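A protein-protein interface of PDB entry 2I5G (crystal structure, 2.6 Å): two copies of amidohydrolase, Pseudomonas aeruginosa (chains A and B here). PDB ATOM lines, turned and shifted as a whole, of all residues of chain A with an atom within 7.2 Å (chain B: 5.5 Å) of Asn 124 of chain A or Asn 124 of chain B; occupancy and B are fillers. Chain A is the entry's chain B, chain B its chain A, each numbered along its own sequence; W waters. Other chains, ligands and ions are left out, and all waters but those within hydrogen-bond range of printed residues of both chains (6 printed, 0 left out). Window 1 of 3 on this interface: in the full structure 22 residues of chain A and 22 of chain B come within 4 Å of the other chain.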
ATOM      1  N   TRP A  44       9.160 -10.592  30.642  1.00  0.00           N
ATOM      2  CA  TRP A  44       8.850 -11.876  30.018  1.00  0.00           C
ATOM      3  C   TRP A  44       9.102 -11.857  28.507  1.00  0.00           C
ATOM      4  O   TRP A  44       9.252 -12.912  27.883  1.00  0.00           O
ATOM      5  CB  TRP A  44       7.387 -12.260  30.253  1.00  0.00           C
ATOM      6  CG  TRP A  44       7.038 -12.759  31.629  1.00  0.00           C
ATOM      7  CD1 TRP A  44       5.983 -12.356  32.392  1.00  0.00           C
ATOM      8  CD2 TRP A  44       7.693 -13.795  32.370  1.00  0.00           C
ATOM      9  NE1 TRP A  44       5.934 -13.075  33.560  1.00  0.00           N
ATOM     10  CE2 TRP A  44       6.973 -13.966  33.575  1.00  0.00           C
ATOM     11  CE3 TRP A  44       8.819 -14.595  32.138  1.00  0.00           C
ATOM     12  CZ2 TRP A  44       7.340 -14.909  34.547  1.00  0.00           C
ATOM     13  CZ3 TRP A  44       9.186 -15.531  33.102  1.00  0.00           C
ATOM     14  CH2 TRP A  44       8.445 -15.679  34.295  1.00  0.00           C
ATOM     15  N   GLN A  93      14.439  -7.060  33.748  1.00  0.00           N
ATOM     16  CA  GLN A  93      14.320  -7.938  34.900  1.00  0.00           C
ATOM     17  C   GLN A  93      14.465  -9.387  34.455  1.00  0.00           C
ATOM     18  O   GLN A  93      14.199 -10.325  35.209  1.00  0.00           O
ATOM     19  CB  GLN A  93      12.988  -7.724  35.608  1.00  0.00           C
ATOM     20  CG  GLN A  93      13.002  -6.528  36.544  1.00  0.00           C
ATOM     21  CD  GLN A  93      12.016  -6.670  37.684  1.00  0.00           C
ATOM     22  OE1 GLN A  93      12.121  -7.591  38.501  1.00  0.00           O
ATOM     23  NE2 GLN A  93      11.048  -5.759  37.749  1.00  0.00           N
ATOM     24  N   ASN A  94      14.914  -9.558  33.218  1.00  0.00           N
ATOM     25  CA  ASN A  94      15.107 -10.880  32.651  1.00  0.00           C
ATOM     26  C   ASN A  94      16.046 -10.786  31.455  1.00  0.00           C
ATOM     27  O   ASN A  94      15.861  -9.939  30.581  1.00  0.00           O
ATOM     28  CB  ASN A  94      13.767 -11.444  32.194  1.00  0.00           C
ATOM     29  CG  ASN A  94      13.825 -12.923  31.913  1.00  0.00           C
ATOM     30  OD1 ASN A  94      14.891 -13.484  31.677  1.00  0.00           O
ATOM     31  ND2 ASN A  94      12.672 -13.566  31.929  1.00  0.00           N
ATOM     32  N   ALA A  95      17.050 -11.655  31.413  1.00  0.00           N
ATOM     33  CA  ALA A  95      17.997 -11.648  30.302  1.00  0.00           C
ATOM     34  C   ALA A  95      17.379 -12.265  29.046  1.00  0.00           C
ATOM     35  O   ALA A  95      18.007 -12.296  27.992  1.00  0.00           O
ATOM     36  CB  ALA A  95      19.256 -12.402  30.688  1.00  0.00           C
ATOM     37  N   HIS A  96      16.146 -12.753  29.166  1.00  0.00           N
ATOM     38  CA  HIS A  96      15.444 -13.367  28.046  1.00  0.00           C
ATOM     39  C   HIS A  96      15.401 -12.459  26.819  1.00  0.00           C
ATOM     40  O   HIS A  96      15.243 -12.931  25.694  1.00  0.00           O
ATOM     41  CB  HIS A  96      14.016 -13.725  28.458  1.00  0.00           C
ATOM     42  CG  HIS A  96      13.193 -14.296  27.348  1.00  0.00           C
ATOM     43  ND1 HIS A  96      13.493 -15.496  26.738  1.00  0.00           N
ATOM     44  CD2 HIS A  96      12.093 -13.819  26.717  1.00  0.00           C
ATOM     45  CE1 HIS A  96      12.614 -15.733  25.780  1.00  0.00           C
ATOM     46  NE2 HIS A  96      11.753 -14.731  25.746  1.00  0.00           N
ATOM     47  N   ALA A  97      15.532 -11.157  27.036  1.00  0.00           N
ATOM     48  CA  ALA A  97      15.504 -10.204  25.932  1.00  0.00           C
ATOM     49  C   ALA A  97      16.719 -10.372  25.017  1.00  0.00           C
ATOM     50  O   ALA A  97      16.677  -9.990  23.846  1.00  0.00           O
ATOM     51  CB  ALA A  97      15.445  -8.791  26.472  1.00  0.00           C
ATOM     52  N   GLN A 117      18.747  -7.958  34.946  1.00  0.00           N
ATOM     53  CA  GLN A 117      18.583  -9.104  35.830  1.00  0.00           C
ATOM     54  C   GLN A 117      18.796 -10.374  35.002  1.00  0.00           C
ATOM     55  O   GLN A 117      18.280 -10.489  33.893  1.00  0.00           O
ATOM     56  CB  GLN A 117      17.179  -9.074  36.432  1.00  0.00           C
ATOM     57  CG  GLN A 117      16.837 -10.265  37.276  1.00  0.00           C
ATOM     58  CD  GLN A 117      15.794  -9.941  38.316  1.00  0.00           C
ATOM     59  OE1 GLN A 117      16.089  -9.920  39.511  1.00  0.00           O
ATOM     60  NE2 GLN A 117      14.569  -9.676  37.871  1.00  0.00           N
ATOM     61  N   MET A 118      19.550 -11.327  35.541  1.00  0.00           N
ATOM     62  CA  MET A 118      19.858 -12.555  34.807  1.00  0.00           C
ATOM     63  C   MET A 118      18.713 -13.510  34.493  1.00  0.00           C
ATOM     64  O   MET A 118      18.700 -14.120  33.427  1.00  0.00           O
ATOM     65  CB  MET A 118      20.975 -13.322  35.517  1.00  0.00           C
ATOM     66  CG  MET A 118      22.267 -13.420  34.698  1.00  0.00           C
ATOM     67  SD  MET A 118      23.032 -11.694  34.230  1.00  0.00           S
ATOM     68  CE  MET A 118      23.124 -11.003  36.019  1.00  0.00           C
ATOM     69  N   CYS A 119      17.759 -13.647  35.409  1.00  0.00           N
ATOM     70  CA  CYS A 119      16.616 -14.542  35.208  1.00  0.00           C
ATOM     71  C   CYS A 119      15.415 -13.966  35.908  1.00  0.00           C
ATOM     72  O   CYS A 119      15.543 -13.100  36.774  1.00  0.00           O
ATOM     73  CB  CYS A 119      16.860 -15.921  35.833  1.00  0.00           C
ATOM     74  SG  CYS A 119      18.387 -16.730  35.412  1.00  0.00           S
ATOM     75  N   TYR A 120      14.240 -14.463  35.555  1.00  0.00           N
ATOM     76  CA  TYR A 120      13.038 -14.003  36.214  1.00  0.00           C
ATOM     77  C   TYR A 120      12.210 -15.190  36.665  1.00  0.00           C
ATOM     78  O   TYR A 120      11.472 -15.778  35.870  1.00  0.00           O
ATOM     79  CB  TYR A 120      12.194 -13.117  35.298  1.00  0.00           C
ATOM     80  CG  TYR A 120      11.094 -12.418  36.063  1.00  0.00           C
ATOM     81  CD1 TYR A 120      11.389 -11.365  36.933  1.00  0.00           C
ATOM     82  CD2 TYR A 120       9.772 -12.861  35.991  1.00  0.00           C
ATOM     83  CE1 TYR A 120      10.397 -10.776  37.716  1.00  0.00           C
ATOM     84  CE2 TYR A 120       8.774 -12.280  36.769  1.00  0.00           C
ATOM     85  CZ  TYR A 120       9.093 -11.239  37.631  1.00  0.00           C
ATOM     86  OH  TYR A 120       8.113 -10.672  38.422  1.00  0.00           O
ATOM     87  N   THR A 122      11.865 -18.312  36.711  1.00  0.00           N
ATOM     88  CA  THR A 122      12.108 -19.669  36.206  1.00  0.00           C
ATOM     89  C   THR A 122      13.352 -19.809  35.329  1.00  0.00           C
ATOM     90  O   THR A 122      14.108 -18.853  35.155  1.00  0.00           O
ATOM     91  CB  THR A 122      10.892 -20.205  35.428  1.00  0.00           C
ATOM     92  OG1 THR A 122      10.675 -19.404  34.262  1.00  0.00           O
ATOM     93  CG2 THR A 122       9.648 -20.169  36.303  1.00  0.00           C
ATOM     94  N   GLN A 123      13.556 -21.002  34.774  1.00  0.00           N
ATOM     95  CA  GLN A 123      14.731 -21.266  33.951  1.00  0.00           C
ATOM     96  C   GLN A 123      14.870 -20.362  32.745  1.00  0.00           C
ATOM     97  O   GLN A 123      13.888 -19.984  32.110  1.00  0.00           O
ATOM     98  CB  GLN A 123      14.776 -22.728  33.498  1.00  0.00           C
ATOM     99  CG  GLN A 123      16.034 -23.055  32.698  1.00  0.00           C
ATOM    100  CD  GLN A 123      16.435 -24.517  32.772  1.00  0.00           C
ATOM    101  OE1 GLN A 123      16.629 -25.063  33.860  1.00  0.00           O
ATOM    102  NE2 GLN A 123      16.574 -25.156  31.613  1.00  0.00           N
ATOM    103  N   ASN A 124      16.121 -20.036  32.441  1.00  0.00           N
ATOM    104  CA  ASN A 124      16.491 -19.155  31.340  1.00  0.00           C
ATOM    105  C   ASN A 124      17.418 -19.870  30.374  1.00  0.00           C
ATOM    106  O   ASN A 124      17.525 -21.092  30.371  1.00  0.00           O
ATOM    107  CB  ASN A 124      17.243 -17.942  31.890  1.00  0.00           C
ATOM    108  CG  ASN A 124      16.563 -16.661  31.569  1.00  0.00           C
ATOM    109  OD1 ASN A 124      15.603 -16.642  30.798  1.00  0.00           O
ATOM    110  ND2 ASN A 124      17.047 -15.571  32.147  1.00  0.00           N
ATOM    111  N   LEU A 125      18.098 -19.079  29.557  1.00  0.00           N
ATOM    112  CA  LEU A 125      19.066 -19.604  28.621  1.00  0.00           C
ATOM    113  C   LEU A 125      20.379 -19.448  29.371  1.00  0.00           C
ATOM    114  O   LEU A 125      21.349 -20.144  29.097  1.00  0.00           O
ATOM    115  CB  LEU A 125      19.085 -18.759  27.350  1.00  0.00           C
ATOM    116  CG  LEU A 125      18.813 -19.453  26.012  1.00  0.00           C
ATOM    117  CD1 LEU A 125      17.625 -20.409  26.100  1.00  0.00           C
ATOM    118  CD2 LEU A 125      18.553 -18.375  24.973  1.00  0.00           C
ATOM    119  N   VAL A 126      20.387 -18.538  30.345  1.00  0.00           N
ATOM    120  CA  VAL A 126      21.583 -18.267  31.136  1.00  0.00           C
ATOM    121  C   VAL A 126      21.551 -18.845  32.553  1.00  0.00           C
ATOM    122  O   VAL A 126      22.602 -19.073  33.161  1.00  0.00           O
ATOM    123  CB  VAL A 126      21.839 -16.755  31.231  1.00  0.00           C
ATOM    124  CG1 VAL A 126      21.996 -16.174  29.840  1.00  0.00           C
ATOM    125  CG2 VAL A 126      20.697 -16.085  31.946  1.00  0.00           C
ATOM    126  N   GLY A 127      20.356 -19.083  33.085  1.00  0.00           N
ATOM    127  CA  GLY A 127      20.276 -19.643  34.423  1.00  0.00           C
ATOM    128  C   GLY A 127      18.879 -20.014  34.869  1.00  0.00           C
ATOM    129  O   GLY A 127      18.012 -20.340  34.056  1.00  0.00           O
ATOM    130  N   THR A 128      18.672 -19.981  36.180  1.00  0.00           N
ATOM    131  CA  THR A 128      17.379 -20.288  36.767  1.00  0.00           C
ATOM    132  C   THR A 128      17.164 -19.276  37.876  1.00  0.00           C
ATOM    133  O   THR A 128      18.126 -18.800  38.480  1.00  0.00           O
ATOM    134  CB  THR A 128      17.351 -21.704  37.364  1.00  0.00           C
ATOM    135  OG1 THR A 128      17.783 -22.645  36.374  1.00  0.00           O
ATOM    136  CG2 THR A 128      15.938 -22.070  37.809  1.00  0.00           C
ATOM    137  N   GLY A 129      15.908 -18.933  38.132  1.00  0.00           N
ATOM    138  CA  GLY A 129      15.612 -17.976  39.182  1.00  0.00           C
ATOM    139  C   GLY A 129      15.000 -18.644  40.393  1.00  0.00           C
ATOM    140  O   GLY A 129      14.704 -19.836  40.355  1.00  0.00           O
ATOM    141  N   GLU A 132      12.152 -22.253  41.618  1.00  0.00           N
ATOM    142  CA  GLU A 132      12.290 -23.544  40.929  1.00  0.00           C
ATOM    143  C   GLU A 132      13.698 -24.111  41.096  1.00  0.00           C
ATOM    144  O   GLU A 132      14.657 -23.358  41.215  1.00  0.00           O
ATOM    145  CB  GLU A 132      11.929 -23.372  39.435  1.00  0.00           C
ATOM    146  CG  GLU A 132      12.511 -24.396  38.465  1.00  0.00           C
ATOM    147  CD  GLU A 132      11.920 -24.290  37.047  1.00  0.00           C
ATOM    148  OE1 GLU A 132      10.852 -24.898  36.790  1.00  0.00           O
ATOM    149  OE2 GLU A 132      12.516 -23.597  36.188  1.00  0.00           O
ATOM    150  N   SER A 138      24.809 -21.187  33.197  1.00  0.00           N
ATOM    151  CA  SER A 138      25.260 -21.986  32.057  1.00  0.00           C
ATOM    152  C   SER A 138      26.422 -21.351  31.288  1.00  0.00           C
ATOM    153  O   SER A 138      26.831 -20.221  31.564  1.00  0.00           O
ATOM    154  CB  SER A 138      24.100 -22.221  31.091  1.00  0.00           C
ATOM    155  OG  SER A 138      23.858 -21.061  30.315  1.00  0.00           O
ATOM    156  N   PHE A 140      26.401 -20.350  28.261  1.00  0.00           N
ATOM    157  CA  PHE A 140      25.894 -19.190  27.541  1.00  0.00           C
ATOM    158  C   PHE A 140      25.767 -18.017  28.520  1.00  0.00           C
ATOM    159  O   PHE A 140      25.971 -16.861  28.155  1.00  0.00           O
ATOM    160  CB  PHE A 140      24.529 -19.496  26.928  1.00  0.00           C
ATOM    161  CG  PHE A 140      23.971 -18.369  26.118  1.00  0.00           C
ATOM    162  CD1 PHE A 140      24.574 -17.994  24.926  1.00  0.00           C
ATOM    163  CD2 PHE A 140      22.847 -17.675  26.550  1.00  0.00           C
ATOM    164  CE1 PHE A 140      24.064 -16.941  24.170  1.00  0.00           C
ATOM    165  CE2 PHE A 140      22.328 -16.623  25.806  1.00  0.00           C
ATOM    166  CZ  PHE A 140      22.937 -16.254  24.614  1.00  0.00           C
ATOM    167  N   LYS A 266       6.362 -17.560  32.071  1.00  0.00           N
ATOM    168  CA  LYS A 266       6.329 -17.015  30.726  1.00  0.00           C
ATOM    169  C   LYS A 266       5.190 -16.001  30.616  1.00  0.00           C
ATOM    170  O   LYS A 266       4.860 -15.543  29.522  1.00  0.00           O
ATOM    171  CB  LYS A 266       6.123 -18.142  29.711  1.00  0.00           C
ATOM    172  CG  LYS A 266       7.171 -19.243  29.772  1.00  0.00           C
ATOM    173  CD  LYS A 266       8.517 -18.757  29.296  1.00  0.00           C
ATOM    174  CE  LYS A 266       9.590 -19.820  29.468  1.00  0.00           C
ATOM    175  NZ  LYS A 266       9.914 -20.088  30.901  1.00  0.00           N
ATOM    176  N   ASN B  94      15.590 -29.679  18.431  1.00  0.00           N
ATOM    177  CA  ASN B  94      15.597 -28.737  19.541  1.00  0.00           C
ATOM    178  C   ASN B  94      14.175 -28.255  19.816  1.00  0.00           C
ATOM    179  O   ASN B  94      13.415 -27.987  18.890  1.00  0.00           O
ATOM    180  CB  ASN B  94      16.480 -27.534  19.207  1.00  0.00           C
ATOM    181  CG  ASN B  94      16.928 -26.775  20.442  1.00  0.00           C
ATOM    182  OD1 ASN B  94      16.267 -26.801  21.479  1.00  0.00           O
ATOM    183  ND2 ASN B  94      18.052 -26.081  20.332  1.00  0.00           N
ATOM    184  N   ALA B  95      13.821 -28.150  21.091  1.00  0.00           N
ATOM    185  CA  ALA B  95      12.497 -27.677  21.472  1.00  0.00           C
ATOM    186  C   ALA B  95      12.476 -26.151  21.445  1.00  0.00           C
ATOM    187  O   ALA B  95      11.426 -25.534  21.621  1.00  0.00           O
ATOM    188  CB  ALA B  95      12.151 -28.170  22.863  1.00  0.00           C
ATOM    189  N   HIS B  96      13.641 -25.551  21.210  1.00  0.00           N
ATOM    190  CA  HIS B  96      13.775 -24.102  21.181  1.00  0.00           C
ATOM    191  C   HIS B  96      12.841 -23.417  20.186  1.00  0.00           C
ATOM    192  O   HIS B  96      12.474 -22.250  20.372  1.00  0.00           O
ATOM    193  CB  HIS B  96      15.223 -23.712  20.890  1.00  0.00           C
ATOM    194  CG  HIS B  96      15.479 -22.241  21.001  1.00  0.00           C
ATOM    195  ND1 HIS B  96      15.243 -21.532  22.160  1.00  0.00           N
ATOM    196  CD2 HIS B  96      15.920 -21.340  20.090  1.00  0.00           C
ATOM    197  CE1 HIS B  96      15.525 -20.257  21.958  1.00  0.00           C
ATOM    198  NE2 HIS B  96      15.937 -20.114  20.710  1.00  0.00           N
ATOM    199  N   MET B 118      14.114 -32.737  22.785  1.00  0.00           N
ATOM    200  CA  MET B 118      13.922 -31.800  23.885  1.00  0.00           C
ATOM    201  C   MET B 118      14.957 -30.685  23.944  1.00  0.00           C
ATOM    202  O   MET B 118      14.612 -29.519  24.119  1.00  0.00           O
ATOM    203  CB  MET B 118      13.907 -32.552  25.216  1.00  0.00           C
ATOM    204  CG  MET B 118      12.600 -32.420  25.978  1.00  0.00           C
ATOM    205  SD  MET B 118      11.070 -32.735  24.840  1.00  0.00           S
ATOM    206  CE  MET B 118      11.601 -34.463  24.186  1.00  0.00           C
ATOM    207  N   CYS B 119      16.226 -31.038  23.796  1.00  0.00           N
ATOM    208  CA  CYS B 119      17.283 -30.045  23.862  1.00  0.00           C
ATOM    209  C   CYS B 119      18.361 -30.369  22.850  1.00  0.00           C
ATOM    210  O   CYS B 119      18.330 -31.429  22.219  1.00  0.00           O
ATOM    211  CB  CYS B 119      17.901 -30.038  25.259  1.00  0.00           C
ATOM    212  SG  CYS B 119      16.706 -29.908  26.618  1.00  0.00           S
ATOM    213  N   TYR B 120      19.318 -29.457  22.704  1.00  0.00           N
ATOM    214  CA  TYR B 120      20.424 -29.660  21.782  1.00  0.00           C
ATOM    215  C   TYR B 120      21.759 -29.227  22.378  1.00  0.00           C
ATOM    216  O   TYR B 120      22.126 -28.056  22.309  1.00  0.00           O
ATOM    217  CB  TYR B 120      20.194 -28.899  20.475  1.00  0.00           C
ATOM    218  CG  TYR B 120      21.140 -29.347  19.383  1.00  0.00           C
ATOM    219  CD1 TYR B 120      20.936 -30.560  18.716  1.00  0.00           C
ATOM    220  CD2 TYR B 120      22.275 -28.603  19.068  1.00  0.00           C
ATOM    221  CE1 TYR B 120      21.840 -31.025  17.767  1.00  0.00           C
ATOM    222  CE2 TYR B 120      23.190 -29.057  18.122  1.00  0.00           C
ATOM    223  CZ  TYR B 120      22.968 -30.271  17.475  1.00  0.00           C
ATOM    224  OH  TYR B 120      23.879 -30.742  16.546  1.00  0.00           O
ATOM    225  N   THR B 122      23.218 -27.907  24.769  1.00  0.00           N
ATOM    226  CA  THR B 122      23.267 -26.978  25.894  1.00  0.00           C
ATOM    227  C   THR B 122      21.909 -26.679  26.535  1.00  0.00           C
ATOM    228  O   THR B 122      20.882 -27.213  26.116  1.00  0.00           O
ATOM    229  CB  THR B 122      23.914 -25.659  25.464  1.00  0.00           C
ATOM    230  OG1 THR B 122      23.333 -25.234  24.228  1.00  0.00           O
ATOM    231  CG2 THR B 122      25.411 -25.833  25.281  1.00  0.00           C
ATOM    232  N   GLN B 123      21.906 -25.815  27.544  1.00  0.00           N
ATOM    233  CA  GLN B 123      20.671 -25.476  28.247  1.00  0.00           C
ATOM    234  C   GLN B 123      19.595 -24.817  27.382  1.00  0.00           C
ATOM    235  O   GLN B 123      19.865 -23.905  26.602  1.00  0.00           O
ATOM    236  CB  GLN B 123      20.978 -24.599  29.462  1.00  0.00           C
ATOM    237  CG  GLN B 123      19.772 -24.295  30.331  1.00  0.00           C
ATOM    238  CD  GLN B 123      20.164 -23.745  31.692  1.00  0.00           C
ATOM    239  OE1 GLN B 123      20.797 -24.437  32.493  1.00  0.00           O
ATOM    240  NE2 GLN B 123      19.795 -22.495  31.959  1.00  0.00           N
ATOM    241  N   ASN B 124      18.370 -25.301  27.562  1.00  0.00           N
ATOM    242  CA  ASN B 124      17.171 -24.859  26.846  1.00  0.00           C
ATOM    243  C   ASN B 124      16.276 -24.120  27.832  1.00  0.00           C
ATOM    244  O   ASN B 124      16.724 -23.702  28.899  1.00  0.00           O
ATOM    245  CB  ASN B 124      16.412 -26.097  26.359  1.00  0.00           C
ATOM    246  CG  ASN B 124      16.100 -26.051  24.897  1.00  0.00           C
ATOM    247  OD1 ASN B 124      15.581 -27.014  24.329  1.00  0.00           O
ATOM    248  ND2 ASN B 124      16.413 -24.927  24.266  1.00  0.00           N
ATOM    249  N   LEU B 125      15.011 -23.954  27.465  1.00  0.00           N
ATOM    250  CA  LEU B 125      14.046 -23.354  28.376  1.00  0.00           C
ATOM    251  C   LEU B 125      13.377 -24.561  29.038  1.00  0.00           C
ATOM    252  O   LEU B 125      12.769 -24.436  30.099  1.00  0.00           O
ATOM    253  CB  LEU B 125      12.967 -22.539  27.643  1.00  0.00           C
ATOM    254  CG  LEU B 125      13.269 -21.153  27.074  1.00  0.00           C
ATOM    255  CD1 LEU B 125      11.991 -20.562  26.511  1.00  0.00           C
ATOM    256  CD2 LEU B 125      13.833 -20.249  28.146  1.00  0.00           C
ATOM    257  N   VAL B 126      13.503 -25.733  28.408  1.00  0.00           N
ATOM    258  CA  VAL B 126      12.881 -26.947  28.938  1.00  0.00           C
ATOM    259  C   VAL B 126      13.816 -27.895  29.693  1.00  0.00           C
ATOM    260  O   VAL B 126      13.414 -28.528  30.667  1.00  0.00           O
ATOM    261  CB  VAL B 126      12.164 -27.738  27.817  1.00  0.00           C
ATOM    262  CG1 VAL B 126      11.290 -26.794  27.008  1.00  0.00           C
ATOM    263  CG2 VAL B 126      13.165 -28.431  26.924  1.00  0.00           C
ATOM    264  N   GLY B 127      15.060 -27.992  29.247  1.00  0.00           N
ATOM    265  CA  GLY B 127      16.014 -28.859  29.912  1.00  0.00           C
ATOM    266  C   GLY B 127      17.420 -28.449  29.534  1.00  0.00           C
ATOM    267  O   GLY B 127      17.649 -27.298  29.172  1.00  0.00           O
ATOM    268  N   THR B 128      18.363 -29.376  29.604  1.00  0.00           N
ATOM    269  CA  THR B 128      19.733 -29.058  29.245  1.00  0.00           C
ATOM    270  C   THR B 128      20.376 -30.207  28.455  1.00  0.00           C
ATOM    271  O   THR B 128      20.130 -31.383  28.732  1.00  0.00           O
ATOM    272  CB  THR B 128      20.555 -28.693  30.517  1.00  0.00           C
ATOM    273  OG1 THR B 128      21.956 -28.661  30.213  1.00  0.00           O
ATOM    274  CG2 THR B 128      20.293 -29.688  31.611  1.00  0.00           C
ATOM    275  N   GLY B 129      21.185 -29.843  27.460  1.00  0.00           N
ATOM    276  CA  GLY B 129      21.843 -30.812  26.600  1.00  0.00           C
ATOM    277  C   GLY B 129      22.902 -31.700  27.222  1.00  0.00           C
ATOM    278  O   GLY B 129      23.139 -31.659  28.427  1.00  0.00           O
HETATM  279  O   HOH W   1      20.163 -23.149  35.272  1.00  0.00           O
HETATM  280  O   HOH W   2      22.327 -22.168  27.079  1.00  0.00           O
HETATM  281  O   HOH W   3      22.999 -24.096  33.846  1.00  0.00           O
HETATM  282  O   HOH W   4      11.620 -22.120  31.427  1.00  0.00           O
HETATM  283  O   HOH W   5      19.416 -26.260  34.899  1.00  0.00           O
HETATM  284  O   HOH W   6      18.212 -27.803  32.724  1.00  0.00           O
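O of Gly 127 of chain B lies within hydrogen-bond range of NE2 of Gln 123 of chain A, at 3.4 Å. NE2 of Gln 123 of chain B is in hydrogen-bond range of O of Asn 124 of chain A, 3.1 Å away. The backbone carbonyl oxygen (O) of Gly 127 of chain A lies within hydrogen-bond range of the side-chain amide nitrogen (NE2) of Gln 123 of chain B (3.5 Å). The backbone carbonyl oxygen (O) of Asn 124 of chain B is in hydrogen-bond range of the side-chain amide nitrogen (NE2) of Gln 123 of chain A, at 3.1 Å. O of Asn 124 of chain A sits close to O of Asn 124 of chain B, 3.1 Å away.
Water W3 bridges the side-chain amide oxygen of Gln 123 of chain B (2.6 Å) and the backbone NH of Ser 138 of chain A (3.5 Å). Water W1 bridges OG1 of Thr 128 of chain A (2.7 Å) and OE1 of Gln 123 of chain B (3.1 Å). Water W4 lies within hydrogen-bond range of the side-chain amino group of Lys 266 of chain A (2.7 Å), the backbone carbonyl oxygen of Leu 125 of chain B (2.9 Å) and the backbone carbonyl oxygen of Gln 123 of chain A (3.2 Å). Water W2 bridges O of Leu 125 of chain A and O of Gln 123 of chain B. Water W5 lies within hydrogen-bond range of the side-chain amide oxygen of Gln 123 of chain A and the side-chain amide oxygen of Gln 123 of chain B. Water W6 lies within hydrogen-bond range of the side-chain amide nitrogen of Gln 123 of chain A (3.3 Å) and the backbone NH of Thr 128 of chain B (3.5 Å).
Asn 124 of chain A touches just these residues of chain B: Gln 123 (3.1 Å) and Asn 124 (3.1 Å). Printed residues of chain B within 4 Å of Gly 127 of chain A: Gln 123. Printed residues of chain B within 4 Å of Lys 266 of chain A: Leu 125 (3.9 Å). Of the printed residues of chain A, Gln 123 of chain B touches Gln 123 (3.6 Å), Asn 124 (3.1 Å) and Gly 127 (3.5 Å). Of chain A, only Gln 123 (3.1 Å) and Asn 124 (3.1 Å) come within 4 Å of Asn 124 of chain B. Printed residues of chain A within 4 Å of Leu 125 of chain B: Gln 123 (3.97 Å) and Lys 266 (3.9 Å). Printed residues of chain A within 4 Å of Gly 127 of chain B: Gln 123 (3.4 Å).
Gln 123 of chain A touches Gln 123 of chain B. Gln 123 of chain A touches Leu 125 of chain B. Lys 266 of chain A touches Leu 125 of chain B (CE to CD1, 3.9 Å).
The side-chain amide nitrogen (ND2) of Asn 124 of chain A sits close to the side-chain sulfur (SG) of Cys 119 of chain A (3.7 Å). The side-chain amide oxygen (OD1) of Asn 124 of chain B lies close to the side-chain amide oxygen (OD1) of Asn 94 of chain B. The side-chain amide oxygen (OD1) of Asn 94 of chain A is in hydrogen-bond range of the side-chain amide nitrogen (ND2) of Asn 124 of chain A (3.0 Å). The side-chain sulfur of Cys 119 of chain B lies close to the backbone NH of Gly 127 of chain B (3.6 Å). The side-chain carboxylate of Glu 132 of chain A lies within hydrogen-bond range of the backbone NH of Gln 123 of chain A (3.1 Å). The side-chain amide oxygen (OD1) of Asn 124 of chain B sits close to the backbone carbonyl oxygen (O) of Met 118 of chain B.
Gln 123 of chain B touches its own counterpart, Gln 123 of chain A. Gln 123 of chain A touches Asn 124 of chain B, and with the chains exchanged Asn 124 of chain A touches Gln 123 of chain B. Gln 123 of chain A touches Gly 127 of chain B, and with the chains exchanged Gly 127 of chain A touches Gln 123 of chain B. Asn 124 of chain B touches its own counterpart, Asn 124 of chain A. 14 positions are printed for both chains.
Printed residues of chain A that touch a printed residue of chain B: Gln 123, Asn 124, Gly 127 and Lys 266. Printed residues of chain B that touch a printed residue of chain A: Gln 123, Asn 124, Leu 125 and Gly 127. Along chain B the printed residues that touch a printed residue of chain A span positions 123 to 127. Among the printed residues, 8 pairs touch across the chains. Among the printed residues, no Asp or Glu carboxylate lies within 4 Å of a Lys or Arg side-chain nitrogen of the other chain.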
